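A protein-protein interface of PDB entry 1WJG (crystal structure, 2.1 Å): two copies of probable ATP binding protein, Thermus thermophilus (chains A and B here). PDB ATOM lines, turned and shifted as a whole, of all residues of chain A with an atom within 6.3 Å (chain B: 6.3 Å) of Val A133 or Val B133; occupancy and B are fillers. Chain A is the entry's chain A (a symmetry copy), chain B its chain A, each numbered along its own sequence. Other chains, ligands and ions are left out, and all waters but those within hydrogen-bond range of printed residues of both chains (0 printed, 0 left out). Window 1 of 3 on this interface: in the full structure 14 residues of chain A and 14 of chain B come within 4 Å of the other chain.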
ATOM      1  N   LEU A 102      15.198 -10.661  34.923  1.00  0.00           N
ATOM      2  CA  LEU A 102      15.933 -10.133  33.786  1.00  0.00           C
ATOM      3  C   LEU A 102      16.098  -8.632  33.917  1.00  0.00           C
ATOM      4  O   LEU A 102      15.154  -7.925  34.270  1.00  0.00           O
ATOM      5  CB  LEU A 102      15.165 -10.413  32.488  1.00  0.00           C
ATOM      6  CG  LEU A 102      15.716  -9.761  31.214  1.00  0.00           C
ATOM      7  CD1 LEU A 102      17.038 -10.412  30.835  1.00  0.00           C
ATOM      8  CD2 LEU A 102      14.718  -9.886  30.068  1.00  0.00           C
ATOM      9  N   ILE A 103      17.300  -8.156  33.619  1.00  0.00           N
ATOM     10  CA  ILE A 103      17.582  -6.733  33.641  1.00  0.00           C
ATOM     11  C   ILE A 103      17.839  -6.320  32.192  1.00  0.00           C
ATOM     12  O   ILE A 103      18.583  -6.986  31.474  1.00  0.00           O
ATOM     13  CB  ILE A 103      18.814  -6.409  34.499  1.00  0.00           C
ATOM     14  CG1 ILE A 103      18.538  -6.761  35.962  1.00  0.00           C
ATOM     15  CG2 ILE A 103      19.195  -4.947  34.348  1.00  0.00           C
ATOM     16  CD1 ILE A 103      19.760  -6.687  36.840  1.00  0.00           C
ATOM     17  N   VAL A 104      17.167  -5.265  31.748  1.00  0.00           N
ATOM     18  CA  VAL A 104      17.343  -4.766  30.386  1.00  0.00           C
ATOM     19  C   VAL A 104      17.941  -3.370  30.500  1.00  0.00           C
ATOM     20  O   VAL A 104      17.438  -2.537  31.247  1.00  0.00           O
ATOM     21  CB  VAL A 104      16.000  -4.705  29.626  1.00  0.00           C
ATOM     22  CG1 VAL A 104      16.208  -4.194  28.211  1.00  0.00           C
ATOM     23  CG2 VAL A 104      15.364  -6.083  29.586  1.00  0.00           C
ATOM     24  N   MET A 105      19.041  -3.125  29.797  1.00  0.00           N
ATOM     25  CA  MET A 105      19.682  -1.824  29.884  1.00  0.00           C
ATOM     26  C   MET A 105      20.575  -1.528  28.688  1.00  0.00           C
ATOM     27  O   MET A 105      20.902  -2.420  27.909  1.00  0.00           O
ATOM     28  CB  MET A 105      20.485  -1.726  31.191  1.00  0.00           C
ATOM     29  CG  MET A 105      21.640  -2.733  31.319  1.00  0.00           C
ATOM     30  SD  MET A 105      22.533  -2.688  32.999  1.00  0.00           S
ATOM     31  CE  MET A 105      22.911  -0.845  33.090  1.00  0.00           C
ATOM     32  N   SER A 122      26.576  -0.402  33.411  1.00  0.00           N
ATOM     33  CA  SER A 122      26.292  -1.683  32.781  1.00  0.00           C
ATOM     34  C   SER A 122      27.398  -2.678  33.165  1.00  0.00           C
ATOM     35  O   SER A 122      27.135  -3.865  33.336  1.00  0.00           O
ATOM     36  CB  SER A 122      26.202  -1.523  31.264  1.00  0.00           C
ATOM     37  OG  SER A 122      27.381  -0.917  30.758  1.00  0.00           O
ATOM     38  N   VAL A 125      26.625  -3.981  36.651  1.00  0.00           N
ATOM     39  CA  VAL A 125      25.464  -4.866  36.606  1.00  0.00           C
ATOM     40  C   VAL A 125      25.843  -6.223  36.010  1.00  0.00           C
ATOM     41  O   VAL A 125      25.463  -7.262  36.542  1.00  0.00           O
ATOM     42  CB  VAL A 125      24.295  -4.242  35.801  1.00  0.00           C
ATOM     43  CG1 VAL A 125      23.155  -5.235  35.649  1.00  0.00           C
ATOM     44  CG2 VAL A 125      23.799  -2.990  36.494  1.00  0.00           C
ATOM     45  N   VAL A 126      26.596  -6.208  34.913  1.00  0.00           N
ATOM     46  CA  VAL A 126      27.036  -7.450  34.273  1.00  0.00           C
ATOM     47  C   VAL A 126      27.945  -8.230  35.221  1.00  0.00           C
ATOM     48  O   VAL A 126      27.930  -9.465  35.244  1.00  0.00           O
ATOM     49  CB  VAL A 126      27.771  -7.168  32.935  1.00  0.00           C
ATOM     50  CG1 VAL A 126      28.374  -8.461  32.369  1.00  0.00           C
ATOM     51  CG2 VAL A 126      26.791  -6.583  31.927  1.00  0.00           C
ATOM     52  N   ALA A 129      25.063  -8.805  38.868  1.00  0.00           N
ATOM     53  CA  ALA A 129      23.664  -9.235  38.816  1.00  0.00           C
ATOM     54  C   ALA A 129      23.527 -10.750  38.729  1.00  0.00           C
ATOM     55  O   ALA A 129      24.204 -11.394  37.935  1.00  0.00           O
ATOM     56  CB  ALA A 129      22.944  -8.582  37.641  1.00  0.00           C
ATOM     57  N   CYS A 131      20.683 -12.515  37.904  1.00  0.00           N
ATOM     58  CA  CYS A 131      19.887 -12.807  36.715  1.00  0.00           C
ATOM     59  C   CYS A 131      20.556 -12.381  35.402  1.00  0.00           C
ATOM     60  O   CYS A 131      21.556 -11.664  35.406  1.00  0.00           O
ATOM     61  CB  CYS A 131      18.539 -12.094  36.833  1.00  0.00           C
ATOM     62  SG  CYS A 131      18.680 -10.286  36.754  1.00  0.00           S
ATOM     63  N   PRO A 132      20.004 -12.826  34.258  1.00  0.00           N
ATOM     64  CA  PRO A 132      20.542 -12.482  32.936  1.00  0.00           C
ATOM     65  C   PRO A 132      20.419 -10.980  32.688  1.00  0.00           C
ATOM     66  O   PRO A 132      19.546 -10.325  33.256  1.00  0.00           O
ATOM     67  CB  PRO A 132      19.629 -13.255  31.987  1.00  0.00           C
ATOM     68  CG  PRO A 132      19.251 -14.457  32.790  1.00  0.00           C
ATOM     69  CD  PRO A 132      18.950 -13.852  34.137  1.00  0.00           C
ATOM     70  N   VAL A 133      21.302 -10.446  31.850  1.00  0.00           N
ATOM     71  CA  VAL A 133      21.297  -9.021  31.513  1.00  0.00           C
ATOM     72  C   VAL A 133      21.197  -8.856  30.004  1.00  0.00           C
ATOM     73  O   VAL A 133      22.004  -9.405  29.251  1.00  0.00           O
ATOM     74  CB  VAL A 133      22.577  -8.313  32.010  1.00  0.00           C
ATOM     75  CG1 VAL A 133      22.545  -6.825  31.644  1.00  0.00           C
ATOM     76  CG2 VAL A 133      22.711  -8.479  33.521  1.00  0.00           C
ATOM     77  N   LEU A 134      20.184  -8.118  29.565  1.00  0.00           N
ATOM     78  CA  LEU A 134      19.967  -7.864  28.149  1.00  0.00           C
ATOM     79  C   LEU A 134      20.552  -6.493  27.823  1.00  0.00           C
ATOM     80  O   LEU A 134      20.015  -5.453  28.222  1.00  0.00           O
ATOM     81  CB  LEU A 134      18.475  -7.905  27.817  1.00  0.00           C
ATOM     82  CG  LEU A 134      18.129  -8.430  26.419  1.00  0.00           C
ATOM     83  CD1 LEU A 134      16.618  -8.479  26.236  1.00  0.00           C
ATOM     84  CD2 LEU A 134      18.762  -7.576  25.359  1.00  0.00           C
ATOM     85  N   LEU A 135      21.684  -6.515  27.131  1.00  0.00           N
ATOM     86  CA  LEU A 135      22.407  -5.307  26.752  1.00  0.00           C
ATOM     87  C   LEU A 135      21.981  -4.836  25.380  1.00  0.00           C
ATOM     88  O   LEU A 135      22.133  -5.564  24.399  1.00  0.00           O
ATOM     89  CB  LEU A 135      23.906  -5.609  26.742  1.00  0.00           C
ATOM     90  CG  LEU A 135      24.805  -5.179  27.905  1.00  0.00           C
ATOM     91  CD1 LEU A 135      24.063  -5.009  29.226  1.00  0.00           C
ATOM     92  CD2 LEU A 135      25.945  -6.160  28.005  1.00  0.00           C
ATOM     93  N   VAL A 136      21.500  -3.600  25.291  1.00  0.00           N
ATOM     94  CA  VAL A 136      21.048  -3.084  24.007  1.00  0.00           C
ATOM     95  C   VAL A 136      21.797  -1.848  23.505  1.00  0.00           C
ATOM     96  O   VAL A 136      22.159  -0.974  24.319  1.00  0.00           O
ATOM     97  CB  VAL A 136      19.472  -2.929  23.953  1.00  0.00           C
ATOM     98  CG1 VAL A 136      18.837  -3.189  25.310  1.00  0.00           C
ATOM     99  CG2 VAL A 136      19.041  -1.595  23.377  1.00  0.00           C
ATOM    100  N   LEU B 102      19.028 -10.999  17.926  1.00  0.00           N
ATOM    101  CA  LEU B 102      19.433 -11.158  19.312  1.00  0.00           C
ATOM    102  C   LEU B 102      20.448 -12.276  19.440  1.00  0.00           C
ATOM    103  O   LEU B 102      20.286 -13.342  18.844  1.00  0.00           O
ATOM    104  CB  LEU B 102      18.218 -11.520  20.177  1.00  0.00           C
ATOM    105  CG  LEU B 102      18.506 -11.900  21.634  1.00  0.00           C
ATOM    106  CD1 LEU B 102      18.968 -10.671  22.404  1.00  0.00           C
ATOM    107  CD2 LEU B 102      17.268 -12.500  22.290  1.00  0.00           C
ATOM    108  N   ILE B 103      21.486 -12.027  20.228  1.00  0.00           N
ATOM    109  CA  ILE B 103      22.501 -13.029  20.490  1.00  0.00           C
ATOM    110  C   ILE B 103      22.372 -13.400  21.967  1.00  0.00           C
ATOM    111  O   ILE B 103      22.272 -12.526  22.826  1.00  0.00           O
ATOM    112  CB  ILE B 103      23.914 -12.496  20.211  1.00  0.00           C
ATOM    113  CG1 ILE B 103      24.069 -12.183  18.721  1.00  0.00           C
ATOM    114  CG2 ILE B 103      24.958 -13.496  20.674  1.00  0.00           C
ATOM    115  CD1 ILE B 103      25.342 -11.449  18.389  1.00  0.00           C
ATOM    116  N   VAL B 104      22.303 -14.696  22.249  1.00  0.00           N
ATOM    117  CA  VAL B 104      22.195 -15.172  23.626  1.00  0.00           C
ATOM    118  C   VAL B 104      23.463 -15.964  23.920  1.00  0.00           C
ATOM    119  O   VAL B 104      23.845 -16.836  23.147  1.00  0.00           O
ATOM    120  CB  VAL B 104      20.954 -16.071  23.821  1.00  0.00           C
ATOM    121  CG1 VAL B 104      20.857 -16.546  25.259  1.00  0.00           C
ATOM    122  CG2 VAL B 104      19.697 -15.306  23.446  1.00  0.00           C
ATOM    123  N   MET B 105      24.142 -15.632  25.012  1.00  0.00           N
ATOM    124  CA  MET B 105      25.377 -16.326  25.336  1.00  0.00           C
ATOM    125  C   MET B 105      25.745 -16.213  26.808  1.00  0.00           C
ATOM    126  O   MET B 105      25.189 -15.395  27.537  1.00  0.00           O
ATOM    127  CB  MET B 105      26.519 -15.794  24.455  1.00  0.00           C
ATOM    128  CG  MET B 105      26.849 -14.305  24.652  1.00  0.00           C
ATOM    129  SD  MET B 105      28.169 -13.633  23.456  1.00  0.00           S
ATOM    130  CE  MET B 105      29.517 -14.916  23.743  1.00  0.00           C
ATOM    131  N   SER B 122      32.581 -13.178  24.894  1.00  0.00           N
ATOM    132  CA  SER B 122      31.413 -12.368  25.207  1.00  0.00           C
ATOM    133  C   SER B 122      31.811 -10.886  25.152  1.00  0.00           C
ATOM    134  O   SER B 122      31.015 -10.041  24.750  1.00  0.00           O
ATOM    135  CB  SER B 122      30.861 -12.736  26.583  1.00  0.00           C
ATOM    136  OG  SER B 122      31.875 -12.631  27.569  1.00  0.00           O
ATOM    137  N   VAL B 125      31.835  -9.826  21.502  1.00  0.00           N
ATOM    138  CA  VAL B 125      30.467  -9.760  20.994  1.00  0.00           C
ATOM    139  C   VAL B 125      29.757  -8.510  21.517  1.00  0.00           C
ATOM    140  O   VAL B 125      29.095  -7.808  20.758  1.00  0.00           O
ATOM    141  CB  VAL B 125      29.654 -11.027  21.365  1.00  0.00           C
ATOM    142  CG1 VAL B 125      28.200 -10.874  20.949  1.00  0.00           C
ATOM    143  CG2 VAL B 125      30.256 -12.244  20.695  1.00  0.00           C
ATOM    144  N   VAL B 126      29.901  -8.234  22.811  1.00  0.00           N
ATOM    145  CA  VAL B 126      29.283  -7.050  23.412  1.00  0.00           C
ATOM    146  C   VAL B 126      29.873  -5.785  22.792  1.00  0.00           C
ATOM    147  O   VAL B 126      29.177  -4.780  22.613  1.00  0.00           O
ATOM    148  CB  VAL B 126      29.474  -7.032  24.952  1.00  0.00           C
ATOM    149  CG1 VAL B 126      28.975  -5.705  25.541  1.00  0.00           C
ATOM    150  CG2 VAL B 126      28.700  -8.186  25.576  1.00  0.00           C
ATOM    151  N   ALA B 129      28.817  -6.486  18.283  1.00  0.00           N
ATOM    152  CA  ALA B 129      27.528  -6.927  17.746  1.00  0.00           C
ATOM    153  C   ALA B 129      26.543  -5.776  17.588  1.00  0.00           C
ATOM    154  O   ALA B 129      26.376  -4.966  18.493  1.00  0.00           O
ATOM    155  CB  ALA B 129      26.920  -8.010  18.631  1.00  0.00           C
ATOM    156  N   CYS B 131      23.148  -6.033  17.047  1.00  0.00           N
ATOM    157  CA  CYS B 131      21.947  -6.388  17.800  1.00  0.00           C
ATOM    158  C   CYS B 131      22.179  -6.522  19.310  1.00  0.00           C
ATOM    159  O   CYS B 131      23.319  -6.545  19.774  1.00  0.00           O
ATOM    160  CB  CYS B 131      21.402  -7.714  17.267  1.00  0.00           C
ATOM    161  SG  CYS B 131      22.492  -9.123  17.615  1.00  0.00           S
ATOM    162  N   PRO B 132      21.089  -6.609  20.094  1.00  0.00           N
ATOM    163  CA  PRO B 132      21.176  -6.750  21.553  1.00  0.00           C
ATOM    164  C   PRO B 132      21.836  -8.078  21.919  1.00  0.00           C
ATOM    165  O   PRO B 132      21.778  -9.035  21.147  1.00  0.00           O
ATOM    166  CB  PRO B 132      19.710  -6.748  21.981  1.00  0.00           C
ATOM    167  CG  PRO B 132      19.061  -5.879  20.953  1.00  0.00           C
ATOM    168  CD  PRO B 132      19.692  -6.377  19.679  1.00  0.00           C
ATOM    169  N   VAL B 133      22.467  -8.122  23.088  1.00  0.00           N
ATOM    170  CA  VAL B 133      23.136  -9.331  23.570  1.00  0.00           C
ATOM    171  C   VAL B 133      22.582  -9.708  24.936  1.00  0.00           C
ATOM    172  O   VAL B 133      22.581  -8.898  25.865  1.00  0.00           O
ATOM    173  CB  VAL B 133      24.663  -9.129  23.687  1.00  0.00           C
ATOM    174  CG1 VAL B 133      25.337 -10.410  24.194  1.00  0.00           C
ATOM    175  CG2 VAL B 133      25.242  -8.732  22.332  1.00  0.00           C
ATOM    176  N   LEU B 134      22.086 -10.935  25.044  1.00  0.00           N
ATOM    177  CA  LEU B 134      21.532 -11.439  26.292  1.00  0.00           C
ATOM    178  C   LEU B 134      22.609 -12.272  26.981  1.00  0.00           C
ATOM    179  O   LEU B 134      22.950 -13.374  26.539  1.00  0.00           O
ATOM    180  CB  LEU B 134      20.287 -12.285  26.024  1.00  0.00           C
ATOM    181  CG  LEU B 134      19.206 -12.222  27.110  1.00  0.00           C
ATOM    182  CD1 LEU B 134      17.999 -13.054  26.699  1.00  0.00           C
ATOM    183  CD2 LEU B 134      19.749 -12.696  28.428  1.00  0.00           C
ATOM    184  N   LEU B 135      23.165 -11.702  28.043  1.00  0.00           N
ATOM    185  CA  LEU B 135      24.233 -12.330  28.814  1.00  0.00           C
ATOM    186  C   LEU B 135      23.662 -13.124  29.968  1.00  0.00           C
ATOM    187  O   LEU B 135      22.993 -12.564  30.835  1.00  0.00           O
ATOM    188  CB  LEU B 135      25.160 -11.242  29.355  1.00  0.00           C
ATOM    189  CG  LEU B 135      26.504 -10.944  28.683  1.00  0.00           C
ATOM    190  CD1 LEU B 135      26.556 -11.339  27.211  1.00  0.00           C
ATOM    191  CD2 LEU B 135      26.828  -9.490  28.903  1.00  0.00           C
ATOM    192  N   VAL B 136      23.970 -14.416  30.019  1.00  0.00           N
ATOM    193  CA  VAL B 136      23.441 -15.250  31.089  1.00  0.00           C
ATOM    194  C   VAL B 136      24.495 -15.901  31.985  1.00  0.00           C
ATOM    195  O   VAL B 136      25.561 -16.313  31.484  1.00  0.00           O
ATOM    196  CB  VAL B 136      22.349 -16.270  30.559  1.00  0.00           C
ATOM    197  CG1 VAL B 136      22.252 -16.247  29.041  1.00  0.00           C
ATOM    198  CG2 VAL B 136      22.564 -17.674  31.087  1.00  0.00           C
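Hydrophobic or aromatic side chains of chain B within 4 Å of the printed part of chain A: Val B126, Pro B132, Leu B134 and Leu B135.
Printed residues of chain A that touch a printed residue of chain B: Val A126, Pro A132, Val A133, Leu A134 and Leu A135.
Hydrophobic or aromatic side chains of chain A that line the printed part of chain B: Val A126, Pro A132, Leu A134 and Leu A135.
Among the printed residues, no Asp or Glu carboxylate lies within 4 Å of a Lys or Arg side-chain nitrogen of the other chain.
Among the printed residues, pairs that only touch across the chains: Leu A135 with Pro B132 (3.2 Å), Pro A132 with Leu B135 (3.2 Å), Leu A135 with Leu B135 (3.6 Å), Pro A132 with Leu B134 (3.6 Å), Leu A134 with Pro B132 (3.6 Å), Val A133 with Leu B134 (3.6 Å), Leu A134 with Val B133 (3.6 Å), Leu A135 with Val B126 (3.9 Å) and Val A126 with Leu B135 (3.9 Å).
O of Val B133 is in hydrogen-bond range of N of Leu A135 (2.8 Å).
The backbone carbonyl oxygen of Val A133 sits close to the backbone carbonyl oxygen of Val B133 (3.5 Å).
N of Leu B135 is in hydrogen-bond range of O of Val A133.
Val A126 touches Leu B135, and with the chains exchanged Leu A135 touches Val B126.
Pro A132 touches Leu B134, and with the chains exchanged Leu A134 touches Pro B132.
Pro A132 touches Leu B135, and with the chains exchanged Leu A135 touches Pro B132.
Val A133 touches Leu B134, and with the chains exchanged Leu A134 touches Val B133.
Positions printed for both chains: 102, 103, 104, 105, 122, 125, 126, 129, 131, 132, 133, 134, 135 and 136.
Of the 12 pairs that touch across the chains among the printed residues, 12 have their exchanged pair printed and touching as well.
The backbone carbonyl oxygen of Leu B134 lies within hydrogen-bond range of the backbone NH of Met B105 (3.0 Å).
The backbone carbonyl oxygen of Ile B103 sits at hydrogen-bond distance from the backbone NH of Leu B134 (2.7 Å).
O of Leu A134 lies within hydrogen-bond range of N of Met A105, at 3.0 Å.
The backbone carbonyl oxygen (O) of Ile A103 lies within hydrogen-bond range of the backbone NH (N) of Leu A134 (2.7 Å).
The backbone NH of Ile A103 sits at hydrogen-bond distance from the backbone carbonyl oxygen of Pro A132 (3.1 Å).
The backbone NH (N) of Ile B103 sits at hydrogen-bond distance from the backbone carbonyl oxygen (O) of Pro B132.
Val A133 touches just these residues of chain B: Val B133, Leu B134 and Leu B135.
Of chain A, only Val A133, Leu A134 and Leu A135 come within 4 Å of Val B133.
Of the printed residues of chain B, Val A126 touches Leu B135 (3.9 Å).
Printed residues of chain A within 4 Å of Pro B132: Leu A134 and Leu A135.
Printed residues of chain A within 4 Å of Leu B134: Pro A132 and Val A133.
Of the printed residues of chain B, Pro A132 touches Leu B134 (3.6 Å) and Leu B135 (3.2 Å).
Of the printed residues of chain B, Leu A135 touches Val B126, Pro B132, Val B133 and Leu B135.
Val B136 touches none of the printed residues of chain A.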
